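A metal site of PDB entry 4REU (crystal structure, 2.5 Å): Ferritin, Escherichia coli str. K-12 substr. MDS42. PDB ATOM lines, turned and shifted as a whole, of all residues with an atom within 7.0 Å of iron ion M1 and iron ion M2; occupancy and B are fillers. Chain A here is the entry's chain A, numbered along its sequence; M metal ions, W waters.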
ATOM      1  N   GLN A  12     -13.772 -11.692 -22.960  1.00  0.00           N
ATOM      2  CA  GLN A  12     -13.381 -12.913 -23.585  1.00  0.00           C
ATOM      3  C   GLN A  12     -13.708 -14.138 -22.729  1.00  0.00           C
ATOM      4  O   GLN A  12     -14.066 -15.157 -23.274  1.00  0.00           O
ATOM      5  CB  GLN A  12     -11.893 -12.875 -23.922  1.00  0.00           C
ATOM      6  CG  GLN A  12     -11.388 -14.066 -24.729  1.00  0.00           C
ATOM      7  CD  GLN A  12     -12.005 -14.194 -26.113  1.00  0.00           C
ATOM      8  OE1 GLN A  12     -12.323 -13.207 -26.766  1.00  0.00           O
ATOM      9  NE2 GLN A  12     -12.162 -15.439 -26.571  1.00  0.00           N
ATOM     10  N   LEU A  15     -17.150 -14.739 -23.513  1.00  0.00           N
ATOM     11  CA  LEU A  15     -17.377 -15.318 -24.826  1.00  0.00           C
ATOM     12  C   LEU A  15     -17.130 -16.849 -24.816  1.00  0.00           C
ATOM     13  O   LEU A  15     -17.855 -17.615 -25.456  1.00  0.00           O
ATOM     14  CB  LEU A  15     -16.507 -14.636 -25.873  1.00  0.00           C
ATOM     15  CG  LEU A  15     -16.653 -15.143 -27.314  1.00  0.00           C
ATOM     16  CD1 LEU A  15     -18.083 -14.970 -27.829  1.00  0.00           C
ATOM     17  CD2 LEU A  15     -15.655 -14.398 -28.185  1.00  0.00           C
ATOM     18  N   GLU A  16     -16.149 -17.282 -24.044  1.00  0.00           N
ATOM     19  CA  GLU A  16     -15.837 -18.684 -23.914  1.00  0.00           C
ATOM     20  C   GLU A  16     -16.922 -19.460 -23.172  1.00  0.00           C
ATOM     21  O   GLU A  16     -17.174 -20.634 -23.464  1.00  0.00           O
ATOM     22  CB  GLU A  16     -14.497 -18.866 -23.221  1.00  0.00           C
ATOM     23  CG  GLU A  16     -13.345 -18.166 -23.927  1.00  0.00           C
ATOM     24  CD  GLU A  16     -12.695 -18.943 -25.074  1.00  0.00           C
ATOM     25  OE1 GLU A  16     -11.765 -18.364 -25.665  1.00  0.00           O
ATOM     26  OE2 GLU A  16     -13.062 -20.089 -25.409  1.00  0.00           O
ATOM     27  N   SER A  19     -19.702 -19.891 -25.552  1.00  0.00           N
ATOM     28  CA  SER A  19     -19.304 -20.922 -26.527  1.00  0.00           C
ATOM     29  C   SER A  19     -19.513 -22.327 -25.999  1.00  0.00           C
ATOM     30  O   SER A  19     -19.926 -23.216 -26.716  1.00  0.00           O
ATOM     31  CB  SER A  19     -17.839 -20.718 -26.903  1.00  0.00           C
ATOM     32  OG  SER A  19     -17.683 -19.477 -27.563  1.00  0.00           O
ATOM     33  N   TYR A  23     -22.256 -24.850 -27.796  1.00  0.00           N
ATOM     34  CA  TYR A  23     -21.983 -26.221 -28.286  1.00  0.00           C
ATOM     35  C   TYR A  23     -22.807 -27.283 -27.563  1.00  0.00           C
ATOM     36  O   TYR A  23     -23.096 -28.287 -28.136  1.00  0.00           O
ATOM     37  CB  TYR A  23     -20.454 -26.586 -28.207  1.00  0.00           C
ATOM     38  CG  TYR A  23     -19.563 -25.669 -29.016  1.00  0.00           C
ATOM     39  CD1 TYR A  23     -20.038 -24.995 -30.102  1.00  0.00           C
ATOM     40  CD2 TYR A  23     -18.240 -25.457 -28.654  1.00  0.00           C
ATOM     41  CE1 TYR A  23     -19.235 -24.129 -30.816  1.00  0.00           C
ATOM     42  CE2 TYR A  23     -17.406 -24.590 -29.375  1.00  0.00           C
ATOM     43  CZ  TYR A  23     -17.909 -23.925 -30.460  1.00  0.00           C
ATOM     44  OH  TYR A  23     -17.137 -23.060 -31.228  1.00  0.00           O
ATOM     45  N   HIS A  45     -16.744 -31.002 -26.547  1.00  0.00           N
ATOM     46  CA  HIS A  45     -16.153 -29.727 -26.875  1.00  0.00           C
ATOM     47  C   HIS A  45     -16.684 -28.551 -26.001  1.00  0.00           C
ATOM     48  O   HIS A  45     -15.927 -27.631 -25.583  1.00  0.00           O
ATOM     49  CB  HIS A  45     -16.355 -29.422 -28.360  1.00  0.00           C
ATOM     50  CG  HIS A  45     -15.206 -28.674 -28.896  1.00  0.00           C
ATOM     51  ND1 HIS A  45     -15.189 -27.310 -28.975  1.00  0.00           N
ATOM     52  CD2 HIS A  45     -13.952 -29.078 -29.197  1.00  0.00           C
ATOM     53  CE1 HIS A  45     -14.011 -26.904 -29.386  1.00  0.00           C
ATOM     54  NE2 HIS A  45     -13.238 -27.958 -29.510  1.00  0.00           N
ATOM     55  N   GLU A  48     -14.584 -28.505 -23.226  1.00  0.00           N
ATOM     56  CA  GLU A  48     -13.360 -27.816 -23.518  1.00  0.00           C
ATOM     57  C   GLU A  48     -13.486 -26.297 -23.395  1.00  0.00           C
ATOM     58  O   GLU A  48     -12.622 -25.664 -22.766  1.00  0.00           O
ATOM     59  CB  GLU A  48     -12.790 -28.227 -24.871  1.00  0.00           C
ATOM     60  CG  GLU A  48     -12.123 -29.591 -24.778  1.00  0.00           C
ATOM     61  CD  GLU A  48     -11.639 -30.125 -26.115  1.00  0.00           C
ATOM     62  OE1 GLU A  48     -10.940 -29.360 -26.820  1.00  0.00           O
ATOM     63  OE2 GLU A  48     -11.940 -31.311 -26.450  1.00  0.00           O
ATOM     64  N   GLU A  49     -14.548 -25.705 -23.917  1.00  0.00           N
ATOM     65  CA  GLU A  49     -14.713 -24.258 -23.816  1.00  0.00           C
ATOM     66  C   GLU A  49     -14.863 -23.780 -22.379  1.00  0.00           C
ATOM     67  O   GLU A  49     -14.325 -22.738 -22.010  1.00  0.00           O
ATOM     68  CB  GLU A  49     -15.888 -23.781 -24.617  1.00  0.00           C
ATOM     69  CG  GLU A  49     -15.801 -24.068 -26.094  1.00  0.00           C
ATOM     70  CD  GLU A  49     -14.721 -23.310 -26.810  1.00  0.00           C
ATOM     71  OE1 GLU A  49     -14.217 -22.288 -26.293  1.00  0.00           O
ATOM     72  OE2 GLU A  49     -14.407 -23.735 -27.943  1.00  0.00           O
ATOM     73  N   MET A  50     -15.515 -24.556 -21.537  1.00  0.00           N
ATOM     74  CA  MET A  50     -15.523 -24.251 -20.089  1.00  0.00           C
ATOM     75  C   MET A  50     -14.108 -24.153 -19.542  1.00  0.00           C
ATOM     76  O   MET A  50     -13.834 -23.286 -18.728  1.00  0.00           O
ATOM     77  CB  MET A  50     -16.327 -25.275 -19.301  1.00  0.00           C
ATOM     78  CG  MET A  50     -17.108 -24.708 -18.121  1.00  0.00           C
ATOM     79  SD  MET A  50     -18.477 -23.554 -18.465  1.00  0.00           S
ATOM     80  CE  MET A  50     -17.545 -22.108 -18.069  1.00  0.00           C
ATOM     81  N   HIS A  52     -11.408 -23.267 -21.204  1.00  0.00           N
ATOM     82  CA  HIS A  52     -10.964 -21.969 -21.735  1.00  0.00           C
ATOM     83  C   HIS A  52     -11.474 -20.795 -20.866  1.00  0.00           C
ATOM     84  O   HIS A  52     -10.758 -19.880 -20.537  1.00  0.00           O
ATOM     85  CB  HIS A  52     -11.436 -21.769 -23.192  1.00  0.00           C
ATOM     86  CG  HIS A  52     -10.980 -22.846 -24.122  1.00  0.00           C
ATOM     87  ND1 HIS A  52     -11.290 -22.849 -25.471  1.00  0.00           N
ATOM     88  CD2 HIS A  52     -10.218 -23.950 -23.909  1.00  0.00           C
ATOM     89  CE1 HIS A  52     -10.759 -23.917 -26.036  1.00  0.00           C
ATOM     90  NE2 HIS A  52     -10.103 -24.603 -25.111  1.00  0.00           N
ATOM     91  N   MET A  53     -12.730 -20.864 -20.501  1.00  0.00           N
ATOM     92  CA  MET A  53     -13.328 -19.870 -19.683  1.00  0.00           C
ATOM     93  C   MET A  53     -12.619 -19.836 -18.338  1.00  0.00           C
ATOM     94  O   MET A  53     -12.210 -18.752 -17.907  1.00  0.00           O
ATOM     95  CB  MET A  53     -14.817 -20.170 -19.570  1.00  0.00           C
ATOM     96  CG  MET A  53     -15.650 -19.200 -18.755  1.00  0.00           C
ATOM     97  SD  MET A  53     -15.610 -19.712 -17.028  1.00  0.00           S
ATOM     98  CE  MET A  53     -17.261 -19.273 -16.499  1.00  0.00           C
ATOM     99  N   HIS A  92     -18.130 -19.308 -35.726  1.00  0.00           N
ATOM    100  CA  HIS A  92     -18.059 -18.894 -34.348  1.00  0.00           C
ATOM    101  C   HIS A  92     -16.614 -18.987 -33.895  1.00  0.00           C
ATOM    102  O   HIS A  92     -16.083 -18.045 -33.336  1.00  0.00           O
ATOM    103  CB  HIS A  92     -19.045 -19.645 -33.482  1.00  0.00           C
ATOM    104  CG  HIS A  92     -19.092 -19.160 -32.063  1.00  0.00           C
ATOM    105  ND1 HIS A  92     -19.740 -17.998 -31.702  1.00  0.00           N
ATOM    106  CD2 HIS A  92     -18.512 -19.638 -30.943  1.00  0.00           C
ATOM    107  CE1 HIS A  92     -19.585 -17.814 -30.404  1.00  0.00           C
ATOM    108  NE2 HIS A  92     -18.839 -18.792 -29.914  1.00  0.00           N
ATOM    109  N   GLU A  93     -15.949 -20.069 -34.201  1.00  0.00           N
ATOM    110  CA  GLU A  93     -14.553 -20.174 -33.769  1.00  0.00           C
ATOM    111  C   GLU A  93     -13.703 -19.128 -34.435  1.00  0.00           C
ATOM    112  O   GLU A  93     -12.699 -18.732 -33.867  1.00  0.00           O
ATOM    113  CB  GLU A  93     -13.965 -21.564 -33.980  1.00  0.00           C
ATOM    114  CG  GLU A  93     -14.506 -22.580 -33.018  1.00  0.00           C
ATOM    115  CD  GLU A  93     -13.905 -22.537 -31.646  1.00  0.00           C
ATOM    116  OE1 GLU A  93     -14.553 -22.998 -30.679  1.00  0.00           O
ATOM    117  OE2 GLU A  93     -12.754 -22.092 -31.501  1.00  0.00           O
ATOM    118  N   ILE A  96     -13.997 -16.050 -32.325  1.00  0.00           N
ATOM    119  CA  ILE A  96     -13.202 -16.221 -31.116  1.00  0.00           C
ATOM    120  C   ILE A  96     -11.749 -15.945 -31.437  1.00  0.00           C
ATOM    121  O   ILE A  96     -11.062 -15.253 -30.702  1.00  0.00           O
ATOM    122  CB  ILE A  96     -13.335 -17.663 -30.590  1.00  0.00           C
ATOM    123  CG1 ILE A  96     -14.708 -17.850 -29.987  1.00  0.00           C
ATOM    124  CG2 ILE A  96     -12.290 -17.992 -29.548  1.00  0.00           C
ATOM    125  CD1 ILE A  96     -15.038 -19.280 -29.673  1.00  0.00           C
ATOM    126  N   TRP A 121      -1.329 -18.974 -25.435  1.00  0.00           N
ATOM    127  CA  TRP A 121      -1.954 -20.280 -25.306  1.00  0.00           C
ATOM    128  C   TRP A 121      -3.272 -20.331 -26.104  1.00  0.00           C
ATOM    129  O   TRP A 121      -3.659 -21.357 -26.634  1.00  0.00           O
ATOM    130  CB  TRP A 121      -2.233 -20.563 -23.805  1.00  0.00           C
ATOM    131  CG  TRP A 121      -2.737 -21.913 -23.585  1.00  0.00           C
ATOM    132  CD1 TRP A 121      -2.010 -23.001 -23.261  1.00  0.00           C
ATOM    133  CD2 TRP A 121      -4.097 -22.360 -23.736  1.00  0.00           C
ATOM    134  NE1 TRP A 121      -2.824 -24.116 -23.195  1.00  0.00           N
ATOM    135  CE2 TRP A 121      -4.115 -23.749 -23.484  1.00  0.00           C
ATOM    136  CE3 TRP A 121      -5.312 -21.708 -24.027  1.00  0.00           C
ATOM    137  CZ2 TRP A 121      -5.285 -24.514 -23.505  1.00  0.00           C
ATOM    138  CZ3 TRP A 121      -6.488 -22.458 -24.074  1.00  0.00           C
ATOM    139  CH2 TRP A 121      -6.462 -23.853 -23.811  1.00  0.00           C
ATOM    140  N   TYR A 122      -3.990 -19.225 -26.090  1.00  0.00           N
ATOM    141  CA  TYR A 122      -5.209 -19.094 -26.836  1.00  0.00           C
ATOM    142  C   TYR A 122      -4.898 -18.972 -28.320  1.00  0.00           C
ATOM    143  O   TYR A 122      -5.626 -19.513 -29.158  1.00  0.00           O
ATOM    144  CB  TYR A 122      -6.012 -17.872 -26.339  1.00  0.00           C
ATOM    145  CG  TYR A 122      -6.655 -18.107 -24.995  1.00  0.00           C
ATOM    146  CD1 TYR A 122      -5.986 -17.795 -23.832  1.00  0.00           C
ATOM    147  CD2 TYR A 122      -7.956 -18.630 -24.884  1.00  0.00           C
ATOM    148  CE1 TYR A 122      -6.547 -18.031 -22.600  1.00  0.00           C
ATOM    149  CE2 TYR A 122      -8.510 -18.887 -23.654  1.00  0.00           C
ATOM    150  CZ  TYR A 122      -7.797 -18.582 -22.516  1.00  0.00           C
ATOM    151  OH  TYR A 122      -8.291 -18.795 -21.248  1.00  0.00           O
ATOM    152  N   GLU A 125      -4.122 -22.394 -29.471  1.00  0.00           N
ATOM    153  CA  GLU A 125      -5.369 -23.148 -29.377  1.00  0.00           C
ATOM    154  C   GLU A 125      -6.359 -22.828 -30.435  1.00  0.00           C
ATOM    155  O   GLU A 125      -7.019 -23.724 -30.918  1.00  0.00           O
ATOM    156  CB  GLU A 125      -6.054 -23.000 -28.036  1.00  0.00           C
ATOM    157  CG  GLU A 125      -5.750 -24.189 -27.134  1.00  0.00           C
ATOM    158  CD  GLU A 125      -6.528 -25.430 -27.524  1.00  0.00           C
ATOM    159  OE1 GLU A 125      -5.920 -26.520 -27.483  1.00  0.00           O
ATOM    160  OE2 GLU A 125      -7.739 -25.277 -27.860  1.00  0.00           O
ATOM    161  N   GLN A 126      -6.493 -21.559 -30.786  1.00  0.00           N
ATOM    162  CA  GLN A 126      -7.438 -21.180 -31.819  1.00  0.00           C
ATOM    163  C   GLN A 126      -7.036 -21.690 -33.196  1.00  0.00           C
ATOM    164  O   GLN A 126      -7.878 -22.039 -34.004  1.00  0.00           O
ATOM    165  CB  GLN A 126      -7.649 -19.664 -31.845  1.00  0.00           C
ATOM    166  CG  GLN A 126      -8.546 -19.193 -30.709  1.00  0.00           C
ATOM    167  CD  GLN A 126      -9.838 -19.971 -30.619  1.00  0.00           C
ATOM    168  OE1 GLN A 126     -10.096 -20.628 -29.634  1.00  0.00           O
ATOM    169  NE2 GLN A 126     -10.654 -19.894 -31.655  1.00  0.00           N
ATOM    170  N   GLU A 129      -8.282 -25.156 -33.119  1.00  0.00           N
ATOM    171  CA  GLU A 129      -9.723 -25.128 -33.223  1.00  0.00           C
ATOM    172  C   GLU A 129     -10.173 -24.866 -34.671  1.00  0.00           C
ATOM    173  O   GLU A 129     -11.134 -25.483 -35.142  1.00  0.00           O
ATOM    174  CB  GLU A 129     -10.334 -24.062 -32.314  1.00  0.00           C
ATOM    175  CG  GLU A 129     -10.076 -24.249 -30.831  1.00  0.00           C
ATOM    176  CD  GLU A 129     -10.996 -25.277 -30.246  1.00  0.00           C
ATOM    177  OE1 GLU A 129     -10.597 -26.468 -30.209  1.00  0.00           O
ATOM    178  OE2 GLU A 129     -12.111 -24.877 -29.870  1.00  0.00           O
ATOM    179  N   PHE A 133     -12.463 -27.761 -36.811  1.00  0.00           N
ATOM    180  CA  PHE A 133     -13.794 -27.438 -37.318  1.00  0.00           C
ATOM    181  C   PHE A 133     -13.819 -27.320 -38.866  1.00  0.00           C
ATOM    182  O   PHE A 133     -14.771 -27.779 -39.482  1.00  0.00           O
ATOM    183  CB  PHE A 133     -14.384 -26.214 -36.604  1.00  0.00           C
ATOM    184  CG  PHE A 133     -14.868 -26.517 -35.191  1.00  0.00           C
ATOM    185  CD1 PHE A 133     -16.169 -26.971 -34.958  1.00  0.00           C
ATOM    186  CD2 PHE A 133     -14.018 -26.376 -34.094  1.00  0.00           C
ATOM    187  CE1 PHE A 133     -16.607 -27.258 -33.662  1.00  0.00           C
ATOM    188  CE2 PHE A 133     -14.455 -26.666 -32.812  1.00  0.00           C
ATOM    189  CZ  PHE A 133     -15.759 -27.110 -32.596  1.00  0.00           C
HETATM  190 FE    FE M   1     -12.400 -21.453 -26.595  1.00  0.00          FE
HETATM  191 FE    FE M   2     -13.260 -23.173 -29.315  1.00  0.00          FE
HETATM  192  O   HOH W   1     -10.530 -20.193 -26.803  1.00  0.00           O
HETATM  193  O   HOH W   2     -12.307 -21.654 -28.717  1.00  0.00           O
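The backbone carbonyl oxygen of Glu 93 lies within hydrogen-bond range of the side-chain amide nitrogen of Gln 126 (3.2 Å).
OE1 of Glu 93 sits close to OH of Tyr 23 (2.6 Å).
OE1 of Glu 16 lies within hydrogen-bond range of NE2 of Gln 12 (3.1 Å).
The backbone carbonyl oxygen (O) of His 52 sits at hydrogen-bond distance from the side-chain hydroxyl (OH) of Tyr 122, 2.8 Å away.
A ring nitrogen (NE2) of His 45 is in hydrogen-bond range of the side-chain carboxylate (OE1) of Glu 129, 3.1 Å away.
Gln 126 touches iron ion M1 (OE1 to FE, 3.9 Å).
Of the 20 residues printed, 4 come within 4 Å of iron ion M1.
His 45 touches iron ion M2.
Four residues have an atom within 4 Å of iron ion M2: His 45, Glu 49, Glu 93 and Glu 129.
Along chain A the residues within 4 Å of iron ion M2 span positions 45 to 129.
Iron ion M1 is bound by the side-chain carboxylate (OE2) of Glu 16 (1.9 Å), the side-chain carboxylate (OE1) of Glu 49 (2.0 Å), a ring nitrogen (ND1) of His 52 (2.1 Å), water W2 (2.1 Å) and water W1 (2.3 Å).
Iron ion M1 has five donor atoms within binding distance.
Iron ion M2 is bound by OE2 of Glu 49 (1.9 Å), OE1 of Glu 93 (1.9 Å), water W2 (1.9 Å), OE2 of Glu 129 (2.1 Å) and OE2 of Glu 93 (2.5 Å).
Water W1 bridges the side-chain carboxylate (OE1) of Glu 16 (2.5 Å) and the side-chain amide oxygen (OE1) of Gln 126 (2.9 Å).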
